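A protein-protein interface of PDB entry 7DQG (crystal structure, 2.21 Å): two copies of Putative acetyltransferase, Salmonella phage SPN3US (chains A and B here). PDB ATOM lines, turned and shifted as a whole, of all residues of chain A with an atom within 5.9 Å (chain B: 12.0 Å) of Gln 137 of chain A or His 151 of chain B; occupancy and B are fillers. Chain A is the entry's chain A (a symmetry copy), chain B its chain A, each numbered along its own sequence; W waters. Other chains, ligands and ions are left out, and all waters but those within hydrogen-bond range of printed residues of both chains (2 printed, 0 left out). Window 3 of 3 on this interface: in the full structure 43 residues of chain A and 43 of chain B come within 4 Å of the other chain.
ND1 of His 151 of chain B lies close to OE1 of Gln 137 of chain A (3.4 Å).
N of Tyr 139 of chain A lies within hydrogen-bond range of O of Tyr 131 of chain A (3.1 Å). OD2 of Asp 135 of chain A is in hydrogen-bond range of NE2 of Gln 137 of chain A. OH of Tyr 139 of chain A sits at hydrogen-bond distance from OE1 of Gln 137 of chain A, at 3.3 Å. A ring nitrogen (ND1) of His 110 of chain A sits at hydrogen-bond distance from the side-chain hydroxyl of Thr 112 of chain A, at 2.6 Å.
Among the printed residues, merely in contact across the chains: His 110 of chain A with His 151 of chain B (3.99 Å), Thr 112 of chain A with His 121 of chain B (3.8 Å), Thr 112 of chain A with Gln 126 of chain B (3.9 Å), Thr 112 of chain A with Ile 148 of chain B (3.9 Å), Thr 112 of chain A with Ser 149 of chain B (3.6 Å), Thr 112 of chain A with Ser 150 of chain B (3.9 Å), Thr 112 of chain A with His 151 of chain B (3.7 Å), Tyr 131 of chain A with Trp 130 of chain B (3.9 Å) and Arg 138 of chain A with Ile 148 of chain B (3.7 Å).
Of the printed residues of chain B, Gln 137 of chain A touches His 151 (3.1 Å). Of the printed residues of chain A, His 151 of chain B touches His 110 (3.99 Å), Thr 112 (3.7 Å) and Gln 137 (3.1 Å). Of chain B, only His 121, Gln 126, Ile 148, Ser 149, Ser 150 and His 151 come within 4 Å of Thr 112 of chain A. Tyr 131 of chain A touches one residue of chain B. Ala 133 of chain A touches none of the printed residues of chain B. No residue of chain B comes within 4 Å of Ala 134 of chain A. Asp 135 of chain A touches none of the printed residues of chain B. Of chain B, only Ile 148 comes within 4 Å of Arg 138 of chain A. No residue of chain B comes within 4 Å of Tyr 139 of chain A. Of the printed residues of chain B, His 110 of chain A touches His 151. Of the printed residues of chain A, Gln 126 of chain B touches Thr 112 (3.9 Å). Printed residues of chain A within 4 Å of Ser 149 of chain B: Thr 112 (3.6 Å). Printed residues of chain A within 4 Å of His 121 of chain B: Thr 112. Val 147 of chain B touches none of the printed residues of chain A. Glu 155 of chain B touches none of the printed residues of chain A. The nearest printed residue of chain A that does not touch His 151 of chain B is Tyr 139 of chain A (4.5 Å). The nearest printed residue of chain A that does not touch Ser 149 of chain B is Arg 138 of chain A (4.2 Å).
Of the 11 printed residues of chain A, 5 touch a printed residue of chain B. Of the 17 printed residues of chain B, 7 touch a printed residue of chain A. Printed residues of chain B that touch a printed residue of chain A: His 121, Gln 126, Trp 130, Ile 148, Ser 149, Ser 150 and His 151. Hydrophobic or aromatic side chains of chain B within 4 Å of the printed part of chain A: His 121, Trp 130, Ile 148 and His 151. Among the printed residues, 10 pairs touch across the chains. Among the printed residues, no Asp or Glu carboxylate lies within 4 Å of a Lys or Arg side-chain nitrogen of the other chain.
No position is printed for both chains.
Water W1 lies within hydrogen-bond range of the backbone carbonyl oxygen (O) of Ile 127 of chain B (2.6 Å) and the guanidinium group (NH1) of Arg 138 of chain A (3.0 Å). Water W2 bridges N of Ser 149 of chain B and NH2 of Arg 138 of chain A.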
ATOM      1  N   HIS A 110     -30.643  16.248 -19.756  1.00  0.00           N
ATOM      2  CA  HIS A 110     -30.852  14.809 -19.820  1.00  0.00           C
ATOM      3  C   HIS A 110     -30.914  14.228 -18.406  1.00  0.00           C
ATOM      4  O   HIS A 110     -30.203  14.696 -17.511  1.00  0.00           O
ATOM      5  CB  HIS A 110     -29.734  14.133 -20.615  1.00  0.00           C
ATOM      6  CG  HIS A 110     -30.066  12.743 -21.062  1.00  0.00           C
ATOM      7  ND1 HIS A 110     -29.808  11.630 -20.290  1.00  0.00           N
ATOM      8  CD2 HIS A 110     -30.645  12.287 -22.198  1.00  0.00           C
ATOM      9  CE1 HIS A 110     -30.210  10.548 -20.932  1.00  0.00           C
ATOM     10  NE2 HIS A 110     -30.722  10.919 -22.093  1.00  0.00           N
ATOM     11  N   THR A 112     -29.634  11.674 -17.193  1.00  0.00           N
ATOM     12  CA  THR A 112     -28.353  11.147 -16.738  1.00  0.00           C
ATOM     13  C   THR A 112     -27.392  12.245 -16.299  1.00  0.00           C
ATOM     14  O   THR A 112     -26.421  11.953 -15.593  1.00  0.00           O
ATOM     15  CB  THR A 112     -27.694  10.308 -17.835  1.00  0.00           C
ATOM     16  OG1 THR A 112     -27.576  11.089 -19.030  1.00  0.00           O
ATOM     17  CG2 THR A 112     -28.518   9.056 -18.125  1.00  0.00           C
ATOM     18  N   TYR A 131     -40.287  14.434 -20.738  1.00  0.00           N
ATOM     19  CA  TYR A 131     -40.793  13.939 -22.011  1.00  0.00           C
ATOM     20  C   TYR A 131     -39.742  13.048 -22.658  1.00  0.00           C
ATOM     21  O   TYR A 131     -38.586  12.996 -22.229  1.00  0.00           O
ATOM     22  CB  TYR A 131     -41.169  15.090 -22.949  1.00  0.00           C
ATOM     23  CG  TYR A 131     -39.979  15.857 -23.495  1.00  0.00           C
ATOM     24  CD1 TYR A 131     -39.430  16.919 -22.787  1.00  0.00           C
ATOM     25  CD2 TYR A 131     -39.412  15.523 -24.721  1.00  0.00           C
ATOM     26  CE1 TYR A 131     -38.347  17.624 -23.283  1.00  0.00           C
ATOM     27  CE2 TYR A 131     -38.327  16.221 -25.221  1.00  0.00           C
ATOM     28  CZ  TYR A 131     -37.802  17.271 -24.500  1.00  0.00           C
ATOM     29  OH  TYR A 131     -36.725  17.970 -24.996  1.00  0.00           O
ATOM     30  N   ILE A 132     -40.165  12.355 -23.712  1.00  0.00           N
ATOM     31  CA  ILE A 132     -39.287  11.546 -24.549  1.00  0.00           C
ATOM     32  C   ILE A 132     -39.315  12.142 -25.950  1.00  0.00           C
ATOM     33  O   ILE A 132     -40.390  12.293 -26.544  1.00  0.00           O
ATOM     34  CB  ILE A 132     -39.710  10.069 -24.569  1.00  0.00           C
ATOM     35  CG1 ILE A 132     -39.783   9.518 -23.143  1.00  0.00           C
ATOM     36  CG2 ILE A 132     -38.747   9.250 -25.417  1.00  0.00           C
ATOM     37  CD1 ILE A 132     -40.372   8.128 -23.055  1.00  0.00           C
ATOM     38  N   ALA A 133     -38.140  12.480 -26.474  1.00  0.00           N
ATOM     39  CA  ALA A 133     -38.050  13.146 -27.765  1.00  0.00           C
ATOM     40  C   ALA A 133     -38.351  12.164 -28.897  1.00  0.00           C
ATOM     41  O   ALA A 133     -38.604  10.974 -28.684  1.00  0.00           O
ATOM     42  CB  ALA A 133     -36.670  13.777 -27.941  1.00  0.00           C
ATOM     43  N   ALA A 134     -38.315  12.682 -30.130  1.00  0.00           N
ATOM     44  CA  ALA A 134     -38.665  11.870 -31.291  1.00  0.00           C
ATOM     45  C   ALA A 134     -37.625  10.788 -31.553  1.00  0.00           C
ATOM     46  O   ALA A 134     -37.972   9.677 -31.971  1.00  0.00           O
ATOM     47  CB  ALA A 134     -38.835  12.760 -32.522  1.00  0.00           C
ATOM     48  N   ASP A 135     -36.350  11.088 -31.316  1.00  0.00           N
ATOM     49  CA  ASP A 135     -35.288  10.111 -31.518  1.00  0.00           C
ATOM     50  C   ASP A 135     -35.106   9.173 -30.327  1.00  0.00           C
ATOM     51  O   ASP A 135     -34.145   8.398 -30.311  1.00  0.00           O
ATOM     52  CB  ASP A 135     -33.968  10.822 -31.831  1.00  0.00           C
ATOM     53  CG  ASP A 135     -33.581  11.834 -30.771  1.00  0.00           C
ATOM     54  OD1 ASP A 135     -34.435  12.174 -29.924  1.00  0.00           O
ATOM     55  OD2 ASP A 135     -32.418  12.293 -30.785  1.00  0.00           O
ATOM     56  N   GLY A 136     -35.999   9.227 -29.337  1.00  0.00           N
ATOM     57  CA  GLY A 136     -35.963   8.325 -28.207  1.00  0.00           C
ATOM     58  C   GLY A 136     -35.309   8.876 -26.956  1.00  0.00           C
ATOM     59  O   GLY A 136     -35.410   8.241 -25.899  1.00  0.00           O
ATOM     60  N   GLN A 137     -34.650  10.028 -27.039  1.00  0.00           N
ATOM     61  CA  GLN A 137     -33.966  10.581 -25.878  1.00  0.00           C
ATOM     62  C   GLN A 137     -34.964  11.129 -24.864  1.00  0.00           C
ATOM     63  O   GLN A 137     -36.053  11.592 -25.213  1.00  0.00           O
ATOM     64  CB  GLN A 137     -33.001  11.686 -26.302  1.00  0.00           C
ATOM     65  CG  GLN A 137     -32.264  11.409 -27.601  1.00  0.00           C
ATOM     66  CD  GLN A 137     -30.936  12.135 -27.682  1.00  0.00           C
ATOM     67  OE1 GLN A 137     -30.246  12.304 -26.677  1.00  0.00           O
ATOM     68  NE2 GLN A 137     -30.573  12.573 -28.884  1.00  0.00           N
ATOM     69  N   ARG A 138     -34.576  11.074 -23.593  1.00  0.00           N
ATOM     70  CA  ARG A 138     -35.375  11.604 -22.500  1.00  0.00           C
ATOM     71  C   ARG A 138     -34.814  12.947 -22.049  1.00  0.00           C
ATOM     72  O   ARG A 138     -33.611  13.201 -22.149  1.00  0.00           O
ATOM     73  CB  ARG A 138     -35.397  10.634 -21.320  1.00  0.00           C
ATOM     74  CG  ARG A 138     -35.719   9.205 -21.706  1.00  0.00           C
ATOM     75  CD  ARG A 138     -35.364   8.254 -20.583  1.00  0.00           C
ATOM     76  NE  ARG A 138     -34.188   7.443 -20.895  1.00  0.00           N
ATOM     77  CZ  ARG A 138     -33.013   7.561 -20.283  1.00  0.00           C
ATOM     78  NH1 ARG A 138     -32.847   8.458 -19.320  1.00  0.00           N
ATOM     79  NH2 ARG A 138     -32.000   6.779 -20.633  1.00  0.00           N
ATOM     80  N   TYR A 139     -35.699  13.807 -21.546  1.00  0.00           N
ATOM     81  CA  TYR A 139     -35.287  15.142 -21.143  1.00  0.00           C
ATOM     82  C   TYR A 139     -36.184  15.653 -20.028  1.00  0.00           C
ATOM     83  O   TYR A 139     -37.378  15.340 -19.972  1.00  0.00           O
ATOM     84  CB  TYR A 139     -35.326  16.130 -22.315  1.00  0.00           C
ATOM     85  CG  TYR A 139     -34.237  15.928 -23.341  1.00  0.00           C
ATOM     86  CD1 TYR A 139     -32.944  16.380 -23.110  1.00  0.00           C
ATOM     87  CD2 TYR A 139     -34.502  15.288 -24.544  1.00  0.00           C
ATOM     88  CE1 TYR A 139     -31.945  16.199 -24.048  1.00  0.00           C
ATOM     89  CE2 TYR A 139     -33.510  15.102 -25.489  1.00  0.00           C
ATOM     90  CZ  TYR A 139     -32.234  15.559 -25.236  1.00  0.00           C
ATOM     91  OH  TYR A 139     -31.245  15.373 -26.176  1.00  0.00           O
ATOM     92  N   HIS B 121     -26.422   9.156  -7.583  1.00  0.00           N
ATOM     93  CA  HIS B 121     -25.683   9.150  -8.842  1.00  0.00           C
ATOM     94  C   HIS B 121     -24.196   8.919  -8.606  1.00  0.00           C
ATOM     95  O   HIS B 121     -23.555   8.153  -9.335  1.00  0.00           O
ATOM     96  CB  HIS B 121     -25.909  10.468  -9.583  1.00  0.00           C
ATOM     97  CG  HIS B 121     -25.039  10.645 -10.788  1.00  0.00           C
ATOM     98  ND1 HIS B 121     -25.290  10.014 -11.989  1.00  0.00           N
ATOM     99  CD2 HIS B 121     -23.922  11.389 -10.981  1.00  0.00           C
ATOM    100  CE1 HIS B 121     -24.364  10.359 -12.867  1.00  0.00           C
ATOM    101  NE2 HIS B 121     -23.524  11.193 -12.280  1.00  0.00           N
ATOM    102  N   PHE B 125     -25.843   4.948  -9.244  1.00  0.00           N
ATOM    103  CA  PHE B 125     -27.259   4.757  -9.521  1.00  0.00           C
ATOM    104  C   PHE B 125     -27.715   5.700 -10.628  1.00  0.00           C
ATOM    105  O   PHE B 125     -27.116   6.755 -10.856  1.00  0.00           O
ATOM    106  CB  PHE B 125     -28.101   4.985  -8.261  1.00  0.00           C
ATOM    107  CG  PHE B 125     -28.006   3.870  -7.254  1.00  0.00           C
ATOM    108  CD1 PHE B 125     -26.812   3.602  -6.603  1.00  0.00           C
ATOM    109  CD2 PHE B 125     -29.116   3.093  -6.954  1.00  0.00           C
ATOM    110  CE1 PHE B 125     -26.722   2.576  -5.675  1.00  0.00           C
ATOM    111  CE2 PHE B 125     -29.033   2.067  -6.027  1.00  0.00           C
ATOM    112  CZ  PHE B 125     -27.836   1.808  -5.387  1.00  0.00           C
ATOM    113  N   GLN B 126     -28.782   5.306 -11.322  1.00  0.00           N
ATOM    114  CA  GLN B 126     -29.365   6.115 -12.380  1.00  0.00           C
ATOM    115  C   GLN B 126     -30.882   6.046 -12.288  1.00  0.00           C
ATOM    116  O   GLN B 126     -31.444   5.072 -11.781  1.00  0.00           O
ATOM    117  CB  GLN B 126     -28.912   5.654 -13.777  1.00  0.00           C
ATOM    118  CG  GLN B 126     -27.423   5.821 -14.063  1.00  0.00           C
ATOM    119  CD  GLN B 126     -27.050   7.235 -14.487  1.00  0.00           C
ATOM    120  OE1 GLN B 126     -27.826   8.175 -14.314  1.00  0.00           O
ATOM    121  NE2 GLN B 126     -25.855   7.387 -15.048  1.00  0.00           N
ATOM    122  N   ILE B 127     -31.539   7.093 -12.785  1.00  0.00           N
ATOM    123  CA  ILE B 127     -32.994   7.090 -12.897  1.00  0.00           C
ATOM    124  C   ILE B 127     -33.393   6.149 -14.027  1.00  0.00           C
ATOM    125  O   ILE B 127     -33.018   6.358 -15.188  1.00  0.00           O
ATOM    126  CB  ILE B 127     -33.529   8.506 -13.147  1.00  0.00           C
ATOM    127  CG1 ILE B 127     -33.096   9.457 -12.028  1.00  0.00           C
ATOM    128  CG2 ILE B 127     -35.048   8.490 -13.284  1.00  0.00           C
ATOM    129  CD1 ILE B 127     -33.399  10.912 -12.324  1.00  0.00           C
ATOM    130  N   TRP B 130     -39.932   6.623 -13.973  1.00  0.00           N
ATOM    131  CA  TRP B 130     -40.634   7.748 -13.371  1.00  0.00           C
ATOM    132  C   TRP B 130     -42.134   7.500 -13.452  1.00  0.00           C
ATOM    133  O   TRP B 130     -42.618   6.815 -14.357  1.00  0.00           O
ATOM    134  CB  TRP B 130     -40.245   9.103 -14.018  1.00  0.00           C
ATOM    135  CG  TRP B 130     -40.586   9.324 -15.484  1.00  0.00           C
ATOM    136  CD1 TRP B 130     -41.745   8.994 -16.129  1.00  0.00           C
ATOM    137  CD2 TRP B 130     -39.758   9.969 -16.464  1.00  0.00           C
ATOM    138  NE1 TRP B 130     -41.681   9.374 -17.448  1.00  0.00           N
ATOM    139  CE2 TRP B 130     -40.474   9.976 -17.680  1.00  0.00           C
ATOM    140  CE3 TRP B 130     -38.477  10.533 -16.435  1.00  0.00           C
ATOM    141  CZ2 TRP B 130     -39.951  10.524 -18.852  1.00  0.00           C
ATOM    142  CZ3 TRP B 130     -37.960  11.076 -17.602  1.00  0.00           C
ATOM    143  CH2 TRP B 130     -38.698  11.067 -18.793  1.00  0.00           C
ATOM    144  N   VAL B 147     -28.421  -0.804 -16.726  1.00  0.00           N
ATOM    145  CA  VAL B 147     -29.044  -0.893 -18.040  1.00  0.00           C
ATOM    146  C   VAL B 147     -29.086   0.465 -18.726  1.00  0.00           C
ATOM    147  O   VAL B 147     -28.851   0.564 -19.932  1.00  0.00           O
ATOM    148  CB  VAL B 147     -30.459  -1.501 -17.927  1.00  0.00           C
ATOM    149  CG1 VAL B 147     -31.130  -1.546 -19.297  1.00  0.00           C
ATOM    150  CG2 VAL B 147     -30.399  -2.890 -17.311  1.00  0.00           C
ATOM    151  N   ILE B 148     -29.372   1.522 -17.962  1.00  0.00           N
ATOM    152  CA  ILE B 148     -29.439   2.865 -18.520  1.00  0.00           C
ATOM    153  C   ILE B 148     -28.081   3.255 -19.083  1.00  0.00           C
ATOM    154  O   ILE B 148     -27.044   3.092 -18.427  1.00  0.00           O
ATOM    155  CB  ILE B 148     -29.903   3.862 -17.447  1.00  0.00           C
ATOM    156  CG1 ILE B 148     -31.381   3.643 -17.109  1.00  0.00           C
ATOM    157  CG2 ILE B 148     -29.653   5.301 -17.896  1.00  0.00           C
ATOM    158  CD1 ILE B 148     -32.329   4.059 -18.213  1.00  0.00           C
ATOM    159  N   SER B 149     -28.083   3.761 -20.314  1.00  0.00           N
ATOM    160  CA  SER B 149     -26.892   4.342 -20.916  1.00  0.00           C
ATOM    161  C   SER B 149     -26.828   5.829 -20.593  1.00  0.00           C
ATOM    162  O   SER B 149     -27.855   6.515 -20.575  1.00  0.00           O
ATOM    163  CB  SER B 149     -26.895   4.142 -22.434  1.00  0.00           C
ATOM    164  OG  SER B 149     -26.215   2.955 -22.799  1.00  0.00           O
ATOM    165  N   SER B 150     -25.622   6.321 -20.335  1.00  0.00           N
ATOM    166  CA  SER B 150     -25.391   7.742 -20.115  1.00  0.00           C
ATOM    167  C   SER B 150     -24.945   8.387 -21.421  1.00  0.00           C
ATOM    168  O   SER B 150     -24.146   7.814 -22.169  1.00  0.00           O
ATOM    169  CB  SER B 150     -24.345   7.976 -19.026  1.00  0.00           C
ATOM    170  OG  SER B 150     -23.929   9.330 -19.016  1.00  0.00           O
ATOM    171  N   HIS B 151     -25.456   9.587 -21.684  1.00  0.00           N
ATOM    172  CA  HIS B 151     -25.338  10.218 -22.992  1.00  0.00           C
ATOM    173  C   HIS B 151     -24.794  11.630 -22.834  1.00  0.00           C
ATOM    174  O   HIS B 151     -25.419  12.468 -22.175  1.00  0.00           O
ATOM    175  CB  HIS B 151     -26.698  10.232 -23.699  1.00  0.00           C
ATOM    176  CG  HIS B 151     -26.807  11.246 -24.794  1.00  0.00           C
ATOM    177  ND1 HIS B 151     -27.493  12.431 -24.644  1.00  0.00           N
ATOM    178  CD2 HIS B 151     -26.329  11.245 -26.061  1.00  0.00           C
ATOM    179  CE1 HIS B 151     -27.427  13.121 -25.769  1.00  0.00           C
ATOM    180  NE2 HIS B 151     -26.727  12.423 -26.645  1.00  0.00           N
ATOM    181  N   THR B 152     -23.630  11.888 -23.436  1.00  0.00           N
ATOM    182  CA  THR B 152     -23.059  13.228 -23.472  1.00  0.00           C
ATOM    183  C   THR B 152     -23.367  13.862 -24.819  1.00  0.00           C
ATOM    184  O   THR B 152     -23.038  13.269 -25.858  1.00  0.00           O
ATOM    185  CB  THR B 152     -21.552  13.185 -23.241  1.00  0.00           C
ATOM    186  OG1 THR B 152     -21.285  12.910 -21.860  1.00  0.00           O
ATOM    187  CG2 THR B 152     -20.916  14.521 -23.611  1.00  0.00           C
ATOM    188  N   PRO B 153     -23.992  15.042 -24.855  1.00  0.00           N
ATOM    189  CA  PRO B 153     -24.362  15.629 -26.141  1.00  0.00           C
ATOM    190  C   PRO B 153     -23.129  16.012 -26.939  1.00  0.00           C
ATOM    191  O   PRO B 153     -22.073  16.327 -26.365  1.00  0.00           O
ATOM    192  CB  PRO B 153     -25.180  16.872 -25.741  1.00  0.00           C
ATOM    193  CG  PRO B 153     -25.580  16.636 -24.318  1.00  0.00           C
ATOM    194  CD  PRO B 153     -24.460  15.850 -23.720  1.00  0.00           C
ATOM    195  N   PRO B 154     -23.215  16.001 -28.272  1.00  0.00           N
ATOM    196  CA  PRO B 154     -22.028  16.331 -29.075  1.00  0.00           C
ATOM    197  C   PRO B 154     -21.642  17.796 -29.005  1.00  0.00           C
ATOM    198  O   PRO B 154     -20.467  18.125 -29.211  1.00  0.00           O
ATOM    199  CB  PRO B 154     -22.445  15.922 -30.495  1.00  0.00           C
ATOM    200  CG  PRO B 154     -23.932  16.068 -30.495  1.00  0.00           C
ATOM    201  CD  PRO B 154     -24.384  15.681 -29.111  1.00  0.00           C
ATOM    202  N   GLU B 155     -22.590  18.688 -28.711  1.00  0.00           N
ATOM    203  CA  GLU B 155     -22.285  20.114 -28.683  1.00  0.00           C
ATOM    204  C   GLU B 155     -21.374  20.495 -27.523  1.00  0.00           C
ATOM    205  O   GLU B 155     -20.717  21.538 -27.591  1.00  0.00           O
ATOM    206  CB  GLU B 155     -23.579  20.932 -28.622  1.00  0.00           C
ATOM    207  CG  GLU B 155     -24.456  20.636 -27.414  1.00  0.00           C
ATOM    208  CD  GLU B 155     -25.647  19.763 -27.759  1.00  0.00           C
ATOM    209  OE1 GLU B 155     -25.446  18.698 -28.375  1.00  0.00           O
ATOM    210  OE2 GLU B 155     -26.786  20.145 -27.418  1.00  0.00           O
ATOM    211  N   GLU B 156     -21.316  19.679 -26.466  1.00  0.00           N
ATOM    212  CA  GLU B 156     -20.419  19.983 -25.355  1.00  0.00           C
ATOM    213  C   GLU B 156     -18.962  19.954 -25.800  1.00  0.00           C
ATOM    214  O   GLU B 156     -18.162  20.807 -25.394  1.00  0.00           O
ATOM    215  CB  GLU B 156     -20.650  19.001 -24.205  1.00  0.00           C
ATOM    216  CG  GLU B 156     -19.794  19.276 -22.977  1.00  0.00           C
ATOM    217  CD  GLU B 156     -20.222  18.467 -21.765  1.00  0.00           C
ATOM    218  OE1 GLU B 156     -21.444  18.293 -21.560  1.00  0.00           O
ATOM    219  OE2 GLU B 156     -19.335  18.009 -21.013  1.00  0.00           O
ATOM    220  N   LYS B 157     -18.600  18.982 -26.642  1.00  0.00           N
ATOM    221  CA  LYS B 157     -17.234  18.914 -27.152  1.00  0.00           C
ATOM    222  C   LYS B 157     -16.966  20.025 -28.163  1.00  0.00           C
ATOM    223  O   LYS B 157     -15.886  20.629 -28.156  1.00  0.00           O
ATOM    224  CB  LYS B 157     -16.976  17.540 -27.775  1.00  0.00           C
ATOM    225  CG  LYS B 157     -15.541  17.314 -28.247  1.00  0.00           C
ATOM    226  CD  LYS B 157     -14.523  17.833 -27.235  1.00  0.00           C
ATOM    227  CE  LYS B 157     -13.376  18.566 -27.923  1.00  0.00           C
ATOM    228  NZ  LYS B 157     -12.627  19.453 -26.988  1.00  0.00           N
ATOM    229  N   LEU B 158     -17.936  20.311 -29.037  1.00  0.00           N
ATOM    230  CA  LEU B 158     -17.752  21.364 -30.032  1.00  0.00           C
ATOM    231  C   LEU B 158     -17.543  22.719 -29.369  1.00  0.00           C
ATOM    232  O   LEU B 158     -16.664  23.487 -29.775  1.00  0.00           O
ATOM    233  CB  LEU B 158     -18.953  21.416 -30.976  1.00  0.00           C
ATOM    234  CG  LEU B 158     -19.327  20.129 -31.710  1.00  0.00           C
ATOM    235  CD1 LEU B 158     -20.470  20.392 -32.676  1.00  0.00           C
ATOM    236  CD2 LEU B 158     -18.123  19.547 -32.439  1.00  0.00           C
HETATM  237  O   HOH W   1     -31.773   8.158 -16.578  1.00  0.00           O
HETATM  238  O   HOH W   2     -30.748   3.963 -21.877  1.00  0.00           O
